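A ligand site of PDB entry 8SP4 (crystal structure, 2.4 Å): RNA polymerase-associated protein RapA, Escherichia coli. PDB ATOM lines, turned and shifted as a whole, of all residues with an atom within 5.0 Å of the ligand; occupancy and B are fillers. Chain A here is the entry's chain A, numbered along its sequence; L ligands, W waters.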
ATOM      1  N   ARG A  50      23.265  19.313   9.712  1.00  0.00           N
ATOM      2  CA  ARG A  50      22.806  18.861   8.401  1.00  0.00           C
ATOM      3  C   ARG A  50      22.930  17.336   8.319  1.00  0.00           C
ATOM      4  O   ARG A  50      23.814  16.772   7.676  1.00  0.00           O
ATOM      5  CB  ARG A  50      23.590  19.547   7.290  1.00  0.00           C
ATOM      6  CG  ARG A  50      23.126  19.184   5.887  1.00  0.00           C
ATOM      7  CD  ARG A  50      24.305  19.053   4.945  1.00  0.00           C
ATOM      8  NE  ARG A  50      25.130  20.255   4.931  1.00  0.00           N
ATOM      9  CZ  ARG A  50      24.840  21.353   4.240  1.00  0.00           C
ATOM     10  NH1 ARG A  50      23.734  21.396   3.507  1.00  0.00           N
ATOM     11  NH2 ARG A  50      25.640  22.408   4.293  1.00  0.00           N
ATOM     12  N   THR A  51      22.010  16.674   9.023  1.00  0.00           N
ATOM     13  CA  THR A  51      21.945  15.222   9.033  1.00  0.00           C
ATOM     14  C   THR A  51      20.493  14.782   8.923  1.00  0.00           C
ATOM     15  O   THR A  51      19.570  15.557   9.210  1.00  0.00           O
ATOM     16  CB  THR A  51      22.565  14.614  10.310  1.00  0.00           C
ATOM     17  OG1 THR A  51      21.733  14.932  11.431  1.00  0.00           O
ATOM     18  CG2 THR A  51      23.966  15.134  10.553  1.00  0.00           C
ATOM     19  N   SER A  52      20.303  13.540   8.506  1.00  0.00           N
ATOM     20  CA  SER A  52      19.000  12.918   8.666  1.00  0.00           C
ATOM     21  C   SER A  52      18.794  12.557  10.133  1.00  0.00           C
ATOM     22  O   SER A  52      19.740  12.451  10.920  1.00  0.00           O
ATOM     23  CB  SER A  52      18.881  11.671   7.790  1.00  0.00           C
ATOM     24  OG  SER A  52      19.746  10.645   8.222  1.00  0.00           O
ATOM     25  N   ILE A  54      18.205  10.046  12.451  1.00  0.00           N
ATOM     26  CA  ILE A  54      18.271   8.603  12.724  1.00  0.00           C
ATOM     27  C   ILE A  54      18.174   8.386  14.224  1.00  0.00           C
ATOM     28  O   ILE A  54      18.954   8.972  14.992  1.00  0.00           O
ATOM     29  CB  ILE A  54      19.559   8.004  12.138  1.00  0.00           C
ATOM     30  CG1 ILE A  54      19.706   8.391  10.666  1.00  0.00           C
ATOM     31  CG2 ILE A  54      19.549   6.490  12.286  1.00  0.00           C
ATOM     32  CD1 ILE A  54      20.927   7.821   9.988  1.00  0.00           C
ATOM     33  N   GLN A  57      21.286   7.383  16.560  1.00  0.00           N
ATOM     34  CA  GLN A  57      22.290   8.430  16.699  1.00  0.00           C
ATOM     35  C   GLN A  57      21.824   9.511  17.661  1.00  0.00           C
ATOM     36  O   GLN A  57      22.591   9.983  18.515  1.00  0.00           O
ATOM     37  CB  GLN A  57      22.621   9.034  15.338  1.00  0.00           C
ATOM     38  CG  GLN A  57      23.209   8.035  14.357  1.00  0.00           C
ATOM     39  CD  GLN A  57      23.411   8.637  12.982  1.00  0.00           C
ATOM     40  OE1 GLN A  57      22.902   9.716  12.681  1.00  0.00           O
ATOM     41  NE2 GLN A  57      24.164   7.943  12.142  1.00  0.00           N
ATOM     42  N   GLU A  77      29.225  -0.028  14.947  1.00  0.00           N
ATOM     43  CA  GLU A  77      29.931  -0.674  13.854  1.00  0.00           C
ATOM     44  C   GLU A  77      30.149   0.296  12.699  1.00  0.00           C
ATOM     45  O   GLU A  77      29.674   1.445  12.708  1.00  0.00           O
ATOM     46  CB  GLU A  77      29.164  -1.915  13.390  1.00  0.00           C
ATOM     47  CG  GLU A  77      29.047  -2.991  14.470  1.00  0.00           C
ATOM     48  CD  GLU A  77      28.462  -4.288  13.953  1.00  0.00           C
ATOM     49  OE1 GLU A  77      27.775  -4.263  12.907  1.00  0.00           O
ATOM     50  OE2 GLU A  77      28.687  -5.337  14.603  1.00  0.00           O
ATOM     51  N   VAL A  78      30.884  -0.163  11.685  1.00  0.00           N
ATOM     52  CA  VAL A  78      31.332   0.709  10.608  1.00  0.00           C
ATOM     53  C   VAL A  78      30.136   1.268   9.856  1.00  0.00           C
ATOM     54  O   VAL A  78      29.201   0.547   9.513  1.00  0.00           O
ATOM     55  CB  VAL A  78      32.285  -0.050   9.675  1.00  0.00           C
ATOM     56  CG1 VAL A  78      31.717  -1.412   9.312  1.00  0.00           C
ATOM     57  CG2 VAL A  78      32.581   0.770   8.429  1.00  0.00           C
ATOM     58  N   GLY A  79      30.167   2.587   9.610  1.00  0.00           N
ATOM     59  CA  GLY A  79      29.134   3.252   8.856  1.00  0.00           C
ATOM     60  C   GLY A  79      27.896   3.634   9.624  1.00  0.00           C
ATOM     61  O   GLY A  79      26.951   4.166   9.027  1.00  0.00           O
ATOM     62  N   LEU A  80      27.864   3.399  10.934  1.00  0.00           N
ATOM     63  CA  LEU A  80      26.671   3.663  11.731  1.00  0.00           C
ATOM     64  C   LEU A  80      26.636   5.080  12.299  1.00  0.00           C
ATOM     65  O   LEU A  80      25.636   5.437  12.943  1.00  0.00           O
ATOM     66  CB  LEU A  80      26.551   2.634  12.858  1.00  0.00           C
ATOM     67  CG  LEU A  80      25.801   1.377  12.412  1.00  0.00           C
ATOM     68  CD1 LEU A  80      26.198   0.175  13.238  1.00  0.00           C
ATOM     69  CD2 LEU A  80      24.300   1.610  12.453  1.00  0.00           C
ATOM     70  N   GLY A  81      27.666   5.880  12.078  1.00  0.00           N
ATOM     71  CA  GLY A  81      27.597   7.299  12.403  1.00  0.00           C
ATOM     72  C   GLY A  81      28.371   7.749  13.621  1.00  0.00           C
ATOM     73  O   GLY A  81      27.902   8.616  14.360  1.00  0.00           O
ATOM     74  N   LYS A  82      29.568   7.185  13.830  1.00  0.00           N
ATOM     75  CA  LYS A  82      30.361   7.587  14.989  1.00  0.00           C
ATOM     76  C   LYS A  82      30.839   9.037  14.863  1.00  0.00           C
ATOM     77  O   LYS A  82      30.877   9.771  15.852  1.00  0.00           O
ATOM     78  CB  LYS A  82      31.548   6.643  15.172  1.00  0.00           C
ATOM     79  CG  LYS A  82      31.176   5.323  15.822  1.00  0.00           C
ATOM     80  CD  LYS A  82      32.400   4.436  16.007  1.00  0.00           C
ATOM     81  CE  LYS A  82      32.961   3.977  14.678  1.00  0.00           C
ATOM     82  NZ  LYS A  82      31.964   3.201  13.885  1.00  0.00           N
ATOM     83  N   THR A  83      31.216   9.456  13.651  1.00  0.00           N
ATOM     84  CA  THR A  83      31.588  10.849  13.440  1.00  0.00           C
ATOM     85  C   THR A  83      30.385  11.770  13.641  1.00  0.00           C
ATOM     86  O   THR A  83      30.519  12.856  14.227  1.00  0.00           O
ATOM     87  CB  THR A  83      32.172  11.049  12.037  1.00  0.00           C
ATOM     88  OG1 THR A  83      33.142  10.018  11.786  1.00  0.00           O
ATOM     89  CG2 THR A  83      32.835  12.407  11.922  1.00  0.00           C
ATOM     90  N   ILE A  84      29.216  11.356  13.169  1.00  0.00           N
ATOM     91  CA  ILE A  84      28.007  12.165  13.338  1.00  0.00           C
ATOM     92  C   ILE A  84      27.619  12.236  14.809  1.00  0.00           C
ATOM     93  O   ILE A  84      27.232  13.292  15.320  1.00  0.00           O
ATOM     94  CB  ILE A  84      26.866  11.608  12.469  1.00  0.00           C
ATOM     95  CG1 ILE A  84      27.298  11.552  11.004  1.00  0.00           C
ATOM     96  CG2 ILE A  84      25.610  12.451  12.630  1.00  0.00           C
ATOM     97  CD1 ILE A  84      27.832  12.855  10.467  1.00  0.00           C
ATOM     98  N   GLN A 113      38.686  14.491   6.522  1.00  0.00           N
ATOM     99  CA  GLN A 113      37.344  13.982   6.723  1.00  0.00           C
ATOM    100  C   GLN A 113      36.649  14.735   7.854  1.00  0.00           C
ATOM    101  O   GLN A 113      35.481  15.134   7.728  1.00  0.00           O
ATOM    102  CB  GLN A 113      37.374  12.487   7.029  1.00  0.00           C
ATOM    103  CG  GLN A 113      36.076  11.951   7.620  1.00  0.00           C
ATOM    104  CD  GLN A 113      36.168  10.493   8.034  1.00  0.00           C
ATOM    105  OE1 GLN A 113      36.933   9.714   7.450  1.00  0.00           O
ATOM    106  NE2 GLN A 113      35.393  10.114   9.042  1.00  0.00           N
ATOM    107  N   TRP A 114      37.341  14.936   8.970  1.00  0.00           N
ATOM    108  CA  TRP A 114      36.728  15.582  10.126  1.00  0.00           C
ATOM    109  C   TRP A 114      36.531  17.075   9.902  1.00  0.00           C
ATOM    110  O   TRP A 114      35.552  17.635  10.402  1.00  0.00           O
ATOM    111  CB  TRP A 114      37.569  15.318  11.367  1.00  0.00           C
ATOM    112  CG  TRP A 114      37.279  13.993  11.989  1.00  0.00           C
ATOM    113  CD1 TRP A 114      37.798  12.781  11.623  1.00  0.00           C
ATOM    114  CD2 TRP A 114      36.385  13.735  13.083  1.00  0.00           C
ATOM    115  NE1 TRP A 114      37.285  11.794  12.427  1.00  0.00           N
ATOM    116  CE2 TRP A 114      36.421  12.355  13.327  1.00  0.00           C
ATOM    117  CE3 TRP A 114      35.577  14.545  13.882  1.00  0.00           C
ATOM    118  CZ2 TRP A 114      35.659  11.755  14.333  1.00  0.00           C
ATOM    119  CZ3 TRP A 114      34.822  13.946  14.881  1.00  0.00           C
ATOM    120  CH2 TRP A 114      34.876  12.573  15.100  1.00  0.00           C
ATOM    121  N   GLU A 117      33.396  17.263   7.660  1.00  0.00           N
ATOM    122  CA  GLU A 117      32.204  16.841   8.388  1.00  0.00           C
ATOM    123  C   GLU A 117      31.800  17.863   9.435  1.00  0.00           C
ATOM    124  O   GLU A 117      30.623  18.224   9.559  1.00  0.00           O
ATOM    125  CB  GLU A 117      32.424  15.465   9.021  1.00  0.00           C
ATOM    126  CG  GLU A 117      31.179  14.589   9.029  1.00  0.00           C
ATOM    127  CD  GLU A 117      30.888  13.987   7.673  1.00  0.00           C
ATOM    128  OE1 GLU A 117      31.449  12.918   7.368  1.00  0.00           O
ATOM    129  OE2 GLU A 117      30.112  14.592   6.910  1.00  0.00           O
ATOM    130  N   ARG A 121      28.450  19.920   8.189  1.00  0.00           N
ATOM    131  CA  ARG A 121      27.301  19.318   8.860  1.00  0.00           C
ATOM    132  C   ARG A 121      26.978  19.940  10.204  1.00  0.00           C
ATOM    133  O   ARG A 121      25.820  19.940  10.601  1.00  0.00           O
ATOM    134  CB  ARG A 121      27.522  17.811   9.049  1.00  0.00           C
ATOM    135  CG  ARG A 121      27.618  17.048   7.751  1.00  0.00           C
ATOM    136  CD  ARG A 121      27.223  15.595   7.913  1.00  0.00           C
ATOM    137  NE  ARG A 121      27.550  14.817   6.717  1.00  0.00           N
ATOM    138  CZ  ARG A 121      26.775  14.751   5.637  1.00  0.00           C
ATOM    139  NH1 ARG A 121      25.625  15.408   5.599  1.00  0.00           N
ATOM    140  NH2 ARG A 121      27.157  14.029   4.588  1.00  0.00           N
ATOM    141  N   ASP A 179      39.448   9.559  17.299  1.00  0.00           N
ATOM    142  CA  ASP A 179      38.861   8.656  16.330  1.00  0.00           C
ATOM    143  C   ASP A 179      39.796   7.475  16.071  1.00  0.00           C
ATOM    144  O   ASP A 179      41.013   7.580  16.234  1.00  0.00           O
ATOM    145  CB  ASP A 179      38.556   9.377  15.016  1.00  0.00           C
ATOM    146  CG  ASP A 179      37.609   8.597  14.127  1.00  0.00           C
ATOM    147  OD1 ASP A 179      36.911   7.698  14.641  1.00  0.00           O
ATOM    148  OD2 ASP A 179      37.558   8.887  12.909  1.00  0.00           O
ATOM    149  N   GLU A 180      39.205   6.355  15.655  1.00  0.00           N
ATOM    150  CA  GLU A 180      39.939   5.125  15.387  1.00  0.00           C
ATOM    151  C   GLU A 180      40.859   4.771  16.558  1.00  0.00           C
ATOM    152  O   GLU A 180      42.056   4.523  16.388  1.00  0.00           O
ATOM    153  CB  GLU A 180      40.711   5.215  14.072  1.00  0.00           C
ATOM    154  CG  GLU A 180      39.842   5.368  12.836  1.00  0.00           C
ATOM    155  CD  GLU A 180      39.028   4.114  12.517  1.00  0.00           C
ATOM    156  OE1 GLU A 180      38.010   3.872  13.186  1.00  0.00           O
ATOM    157  OE2 GLU A 180      39.417   3.385  11.586  1.00  0.00           O
ATOM    158  N   LEU A 211      36.473   6.635  19.954  1.00  0.00           N
ATOM    159  CA  LEU A 211      35.715   6.105  18.827  1.00  0.00           C
ATOM    160  C   LEU A 211      36.472   4.932  18.218  1.00  0.00           C
ATOM    161  O   LEU A 211      37.574   5.111  17.691  1.00  0.00           O
ATOM    162  CB  LEU A 211      35.469   7.182  17.767  1.00  0.00           C
ATOM    163  CG  LEU A 211      34.353   8.209  17.954  1.00  0.00           C
ATOM    164  CD1 LEU A 211      34.604   9.133  19.148  1.00  0.00           C
ATOM    165  CD2 LEU A 211      34.170   9.027  16.683  1.00  0.00           C
ATOM    166  N   SER A 466      37.164   9.008   2.232  1.00  0.00           N
ATOM    167  CA  SER A 466      35.938   9.773   2.051  1.00  0.00           C
ATOM    168  C   SER A 466      35.822  10.852   3.117  1.00  0.00           C
ATOM    169  O   SER A 466      36.171  10.649   4.291  1.00  0.00           O
ATOM    170  CB  SER A 466      34.714   8.849   2.110  1.00  0.00           C
ATOM    171  OG  SER A 466      33.518   9.603   2.103  1.00  0.00           O
ATOM    172  N   GLY A 468      32.881  12.226   3.855  1.00  0.00           N
ATOM    173  CA  GLY A 468      31.511  12.205   4.310  1.00  0.00           C
ATOM    174  C   GLY A 468      30.480  12.730   3.347  1.00  0.00           C
ATOM    175  O   GLY A 468      29.283  12.692   3.664  1.00  0.00           O
ATOM    176  N   ARG A 469      30.884  13.216   2.171  1.00  0.00           N
ATOM    177  CA  ARG A 469      29.930  13.725   1.204  1.00  0.00           C
ATOM    178  C   ARG A 469      28.989  12.622   0.747  1.00  0.00           C
ATOM    179  O   ARG A 469      29.414  11.494   0.494  1.00  0.00           O
ATOM    180  CB  ARG A 469      30.653  14.333   0.014  1.00  0.00           C
ATOM    181  CG  ARG A 469      31.734  15.334   0.381  1.00  0.00           C
ATOM    182  CD  ARG A 469      32.532  15.743  -0.830  1.00  0.00           C
ATOM    183  NE  ARG A 469      33.864  16.234  -0.485  1.00  0.00           N
ATOM    184  CZ  ARG A 469      34.129  17.498  -0.164  1.00  0.00           C
ATOM    185  NH1 ARG A 469      33.157  18.399  -0.158  1.00  0.00           N
ATOM    186  NH2 ARG A 469      35.363  17.853   0.147  1.00  0.00           N
ATOM    187  N   ARG A 498      26.020   3.398   2.318  1.00  0.00           N
ATOM    188  CA  ARG A 498      25.715   4.363   3.354  1.00  0.00           C
ATOM    189  C   ARG A 498      24.383   4.032   4.015  1.00  0.00           C
ATOM    190  O   ARG A 498      23.508   3.406   3.410  1.00  0.00           O
ATOM    191  CB  ARG A 498      25.659   5.787   2.779  1.00  0.00           C
ATOM    192  CG  ARG A 498      26.975   6.269   2.204  1.00  0.00           C
ATOM    193  CD  ARG A 498      27.927   6.713   3.305  1.00  0.00           C
ATOM    194  NE  ARG A 498      29.208   7.159   2.779  1.00  0.00           N
ATOM    195  CZ  ARG A 498      29.427   8.369   2.264  1.00  0.00           C
ATOM    196  NH1 ARG A 498      28.447   9.255   2.214  1.00  0.00           N
ATOM    197  NH2 ARG A 498      30.626   8.695   1.817  1.00  0.00           N
ATOM    198  N   ILE A 499      24.248   4.459   5.271  1.00  0.00           N
ATOM    199  CA  ILE A 499      22.983   4.302   5.964  1.00  0.00           C
ATOM    200  C   ILE A 499      21.915   5.133   5.262  1.00  0.00           C
ATOM    201  O   ILE A 499      22.166   6.263   4.825  1.00  0.00           O
ATOM    202  CB  ILE A 499      23.124   4.686   7.451  1.00  0.00           C
ATOM    203  CG1 ILE A 499      21.834   4.381   8.212  1.00  0.00           C
ATOM    204  CG2 ILE A 499      23.521   6.147   7.604  1.00  0.00           C
ATOM    205  CD1 ILE A 499      22.016   4.319   9.712  1.00  0.00           C
ATOM    206  N   LEU A 668      20.341  18.280   2.809  1.00  0.00           N
ATOM    207  CA  LEU A 668      21.059  17.021   2.628  1.00  0.00           C
ATOM    208  C   LEU A 668      21.390  16.781   1.153  1.00  0.00           C
ATOM    209  O   LEU A 668      22.479  16.282   0.837  1.00  0.00           O
ATOM    210  CB  LEU A 668      20.240  15.862   3.196  1.00  0.00           C
ATOM    211  CG  LEU A 668      19.998  15.918   4.699  1.00  0.00           C
ATOM    212  CD1 LEU A 668      19.140  14.762   5.159  1.00  0.00           C
ATOM    213  CD2 LEU A 668      21.316  15.955   5.442  1.00  0.00           C
HETATM  214  P1  LIG L   1      34.096   6.751  11.244  1.00  0.00           P
HETATM  215  S1  LIG L   1      35.047   5.045  11.226  1.00  0.00           S
HETATM  216  O1  LIG L   1      34.068   7.350   9.798  1.00  0.00           O
HETATM  217  O2  LIG L   1      34.879   7.731  12.172  1.00  0.00           O
HETATM  218  P2  LIG L   1      31.567   5.614  11.136  1.00  0.00           P
HETATM  219  O3  LIG L   1      32.187   4.444  10.490  1.00  0.00           O
HETATM  220  O4  LIG L   1      30.620   5.216  12.281  1.00  0.00           O
HETATM  221  O5  LIG L   1      32.634   6.601  11.781  1.00  0.00           O
HETATM  222  P3  LIG L   1      30.627   7.948   9.959  1.00  0.00           P
HETATM  223  O6  LIG L   1      30.181   8.591  11.221  1.00  0.00           O
HETATM  224  O7  LIG L   1      31.989   8.426   9.469  1.00  0.00           O
HETATM  225  O8  LIG L   1      30.674   6.368  10.076  1.00  0.00           O
HETATM  226  O9  LIG L   1      29.512   8.164   8.872  1.00  0.00           O
HETATM  227  C1  LIG L   1      29.432   7.269   7.743  1.00  0.00           C
HETATM  228  C2  LIG L   1      28.915   8.003   6.536  1.00  0.00           C
HETATM  229  O10 LIG L   1      27.479   8.145   6.631  1.00  0.00           O
HETATM  230  C3  LIG L   1      29.468   9.413   6.340  1.00  0.00           C
HETATM  231  O11 LIG L   1      29.628   9.711   4.955  1.00  0.00           O
HETATM  232  C4  LIG L   1      28.398  10.300   6.991  1.00  0.00           C
HETATM  233  O12 LIG L   1      28.343  11.592   6.391  1.00  0.00           O
HETATM  234  C5  LIG L   1      27.121   9.515   6.703  1.00  0.00           C
HETATM  235  N1  LIG L   1      26.098   9.654   7.737  1.00  0.00           N
HETATM  236  C6  LIG L   1      26.058   9.008   8.943  1.00  0.00           C
HETATM  237  N2  LIG L   1      25.025   9.335   9.686  1.00  0.00           N
HETATM  238  C7  LIG L   1      24.343  10.266   8.921  1.00  0.00           C
HETATM  239  C8  LIG L   1      23.167  10.999   9.137  1.00  0.00           C
HETATM  240  N3  LIG L   1      22.436  10.907  10.251  1.00  0.00           N
HETATM  241  N4  LIG L   1      22.761  11.850   8.164  1.00  0.00           N
HETATM  242  C9  LIG L   1      23.495  11.951   7.055  1.00  0.00           C
HETATM  243  N5  LIG L   1      24.627  11.307   6.731  1.00  0.00           N
HETATM  244  C10 LIG L   1      25.003  10.473   7.716  1.00  0.00           C
HETATM  245  O   HOH W   1      37.149   6.730  10.885  1.00  0.00           O
HETATM  246  O   HOH W   2      32.616   4.536   8.009  1.00  0.00           O
HETATM  247  O   HOH W   3      35.821   5.661  13.683  1.00  0.00           O
HETATM  248  O   HOH W   4      26.524   5.319   6.640  1.00  0.00           O
HETATM  249  O   HOH W   5      21.540   9.575   6.085  1.00  0.00           O
HETATM  250  O   HOH W   6      25.893  11.687   4.177  1.00  0.00           O
HETATM  251  O   HOH W   7      20.802  11.401  13.215  1.00  0.00           O
HETATM  252  O   HOH W   8      32.341  10.584   7.744  1.00  0.00           O
HETATM  253  O   HOH W   9      34.138   2.432  12.068  1.00  0.00           O
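OE1 of Glu 180 sits close to S1 of the ligand (3.7 Å).
Merely in contact with the ligand: Thr 51, Ile 54, Glu 77, Val 78, Leu 80, Ile 84 and Glu 117.
Hydrophobic or aromatic side chains within 4 Å of the ligand: Ile 54 and Ile 84.
Of the 26 residues printed, 19 come within 4 Å of the ligand.
The nearest printed residue that does not touch the ligand is Ile 499 (4.1 Å).
OE1 of Gln 113 lies close to O of Ser 466, 3.4 Å away.
The side-chain amino group (NZ) of Lys 82 is in hydrogen-bond range of the backbone carbonyl oxygen (O) of Glu 77, 3.1 Å away.
OG of Ser 466 sits at hydrogen-bond distance from NH2 of Arg 498, at 3.0 Å.
The side-chain amide nitrogen of Gln 57 lies within hydrogen-bond range of the backbone carbonyl oxygen of Leu 80 (3.0 Å).
The backbone NH of Arg 50 is in hydrogen-bond range of the backbone carbonyl oxygen of Arg 121, at 2.8 Å.
NH1 of Arg 498 lies within hydrogen-bond range of O of Arg 469 (3.0 Å).
O of Gly 468 sits at hydrogen-bond distance from NH2 of Arg 121, at 2.7 Å.
N of Glu 180 lies within hydrogen-bond range of O of Leu 211 (2.9 Å).
O of Ser 52 is in hydrogen-bond range of N3 of the ligand, 3.2 Å away.
The side-chain hydroxyl (OG) of Ser 52 is in hydrogen-bond range of a nitrogen (N4) of the ligand, 3.2 Å away.
The backbone NH (N) of Gly 79 is in hydrogen-bond range of an oxygen (O3) of the ligand (2.9 Å).
N of Thr 83 lies within hydrogen-bond range of O6 of the ligand.
N of Ser 52 lies within hydrogen-bond range of N4 of the ligand (3.0 Å).
An oxygen (O11) of the ligand sits close to the guanidinium group (NH1) of Arg 498.
N of Lys 82 is in hydrogen-bond range of O4 of the ligand.
The side-chain amide oxygen (OE1) of Gln 57 lies within hydrogen-bond range of a nitrogen (N3) of the ligand, at 2.7 Å.
The side-chain carboxylate (OD2) of Asp 179 lies within hydrogen-bond range of an oxygen (O2) of the ligand (3.0 Å).
The side-chain amino group (NZ) of Lys 82 lies within salt-bridge range of an oxygen (O4) of the ligand, at 2.9 Å.
O4 of the ligand lies within hydrogen-bond range of N of Gly 81 (3.0 Å).
An oxygen (O1) of the ligand lies within hydrogen-bond range of the side-chain amide nitrogen (NE2) of Gln 113 (3.2 Å).
An oxygen (O2) of the ligand is in hydrogen-bond range of the side-chain hydroxyl (OG1) of Thr 83, at 2.9 Å.
NH2 of Arg 121 is in hydrogen-bond range of O12 of the ligand (3.3 Å).
The backbone carbonyl oxygen (O) of Gly 468 lies within hydrogen-bond range of an oxygen (O12) of the ligand.
Water W8 lies within hydrogen-bond range of OE1 of Glu 117, O7 of the ligand and NE2 of Gln 113.
Water W6 lies within hydrogen-bond range of the guanidinium group of Arg 121 (2.7 Å) and a nitrogen (N5) of the ligand (2.9 Å).
Water W9 bridges a sulfur (S1) of the ligand (2.9 Å) and the side-chain amino group of Lys 82 (2.9 Å).
Water W4 lies within hydrogen-bond range of O of Gly 79 (2.7 Å), N of Ile 499 (2.8 Å) and O10 of the ligand (3.0 Å).
Water W5 bridges the side-chain hydroxyl (OG) of Ser 52 (3.0 Å) and a nitrogen (N4) of the ligand (3.3 Å).
Water W7 lies within hydrogen-bond range of the backbone carbonyl oxygen (O) of Ser 52 (2.7 Å), the side-chain amide oxygen (OE1) of Gln 57 (2.7 Å), the backbone NH (N) of Ile 54 (3.0 Å) and a nitrogen (N3) of the ligand (3.4 Å).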
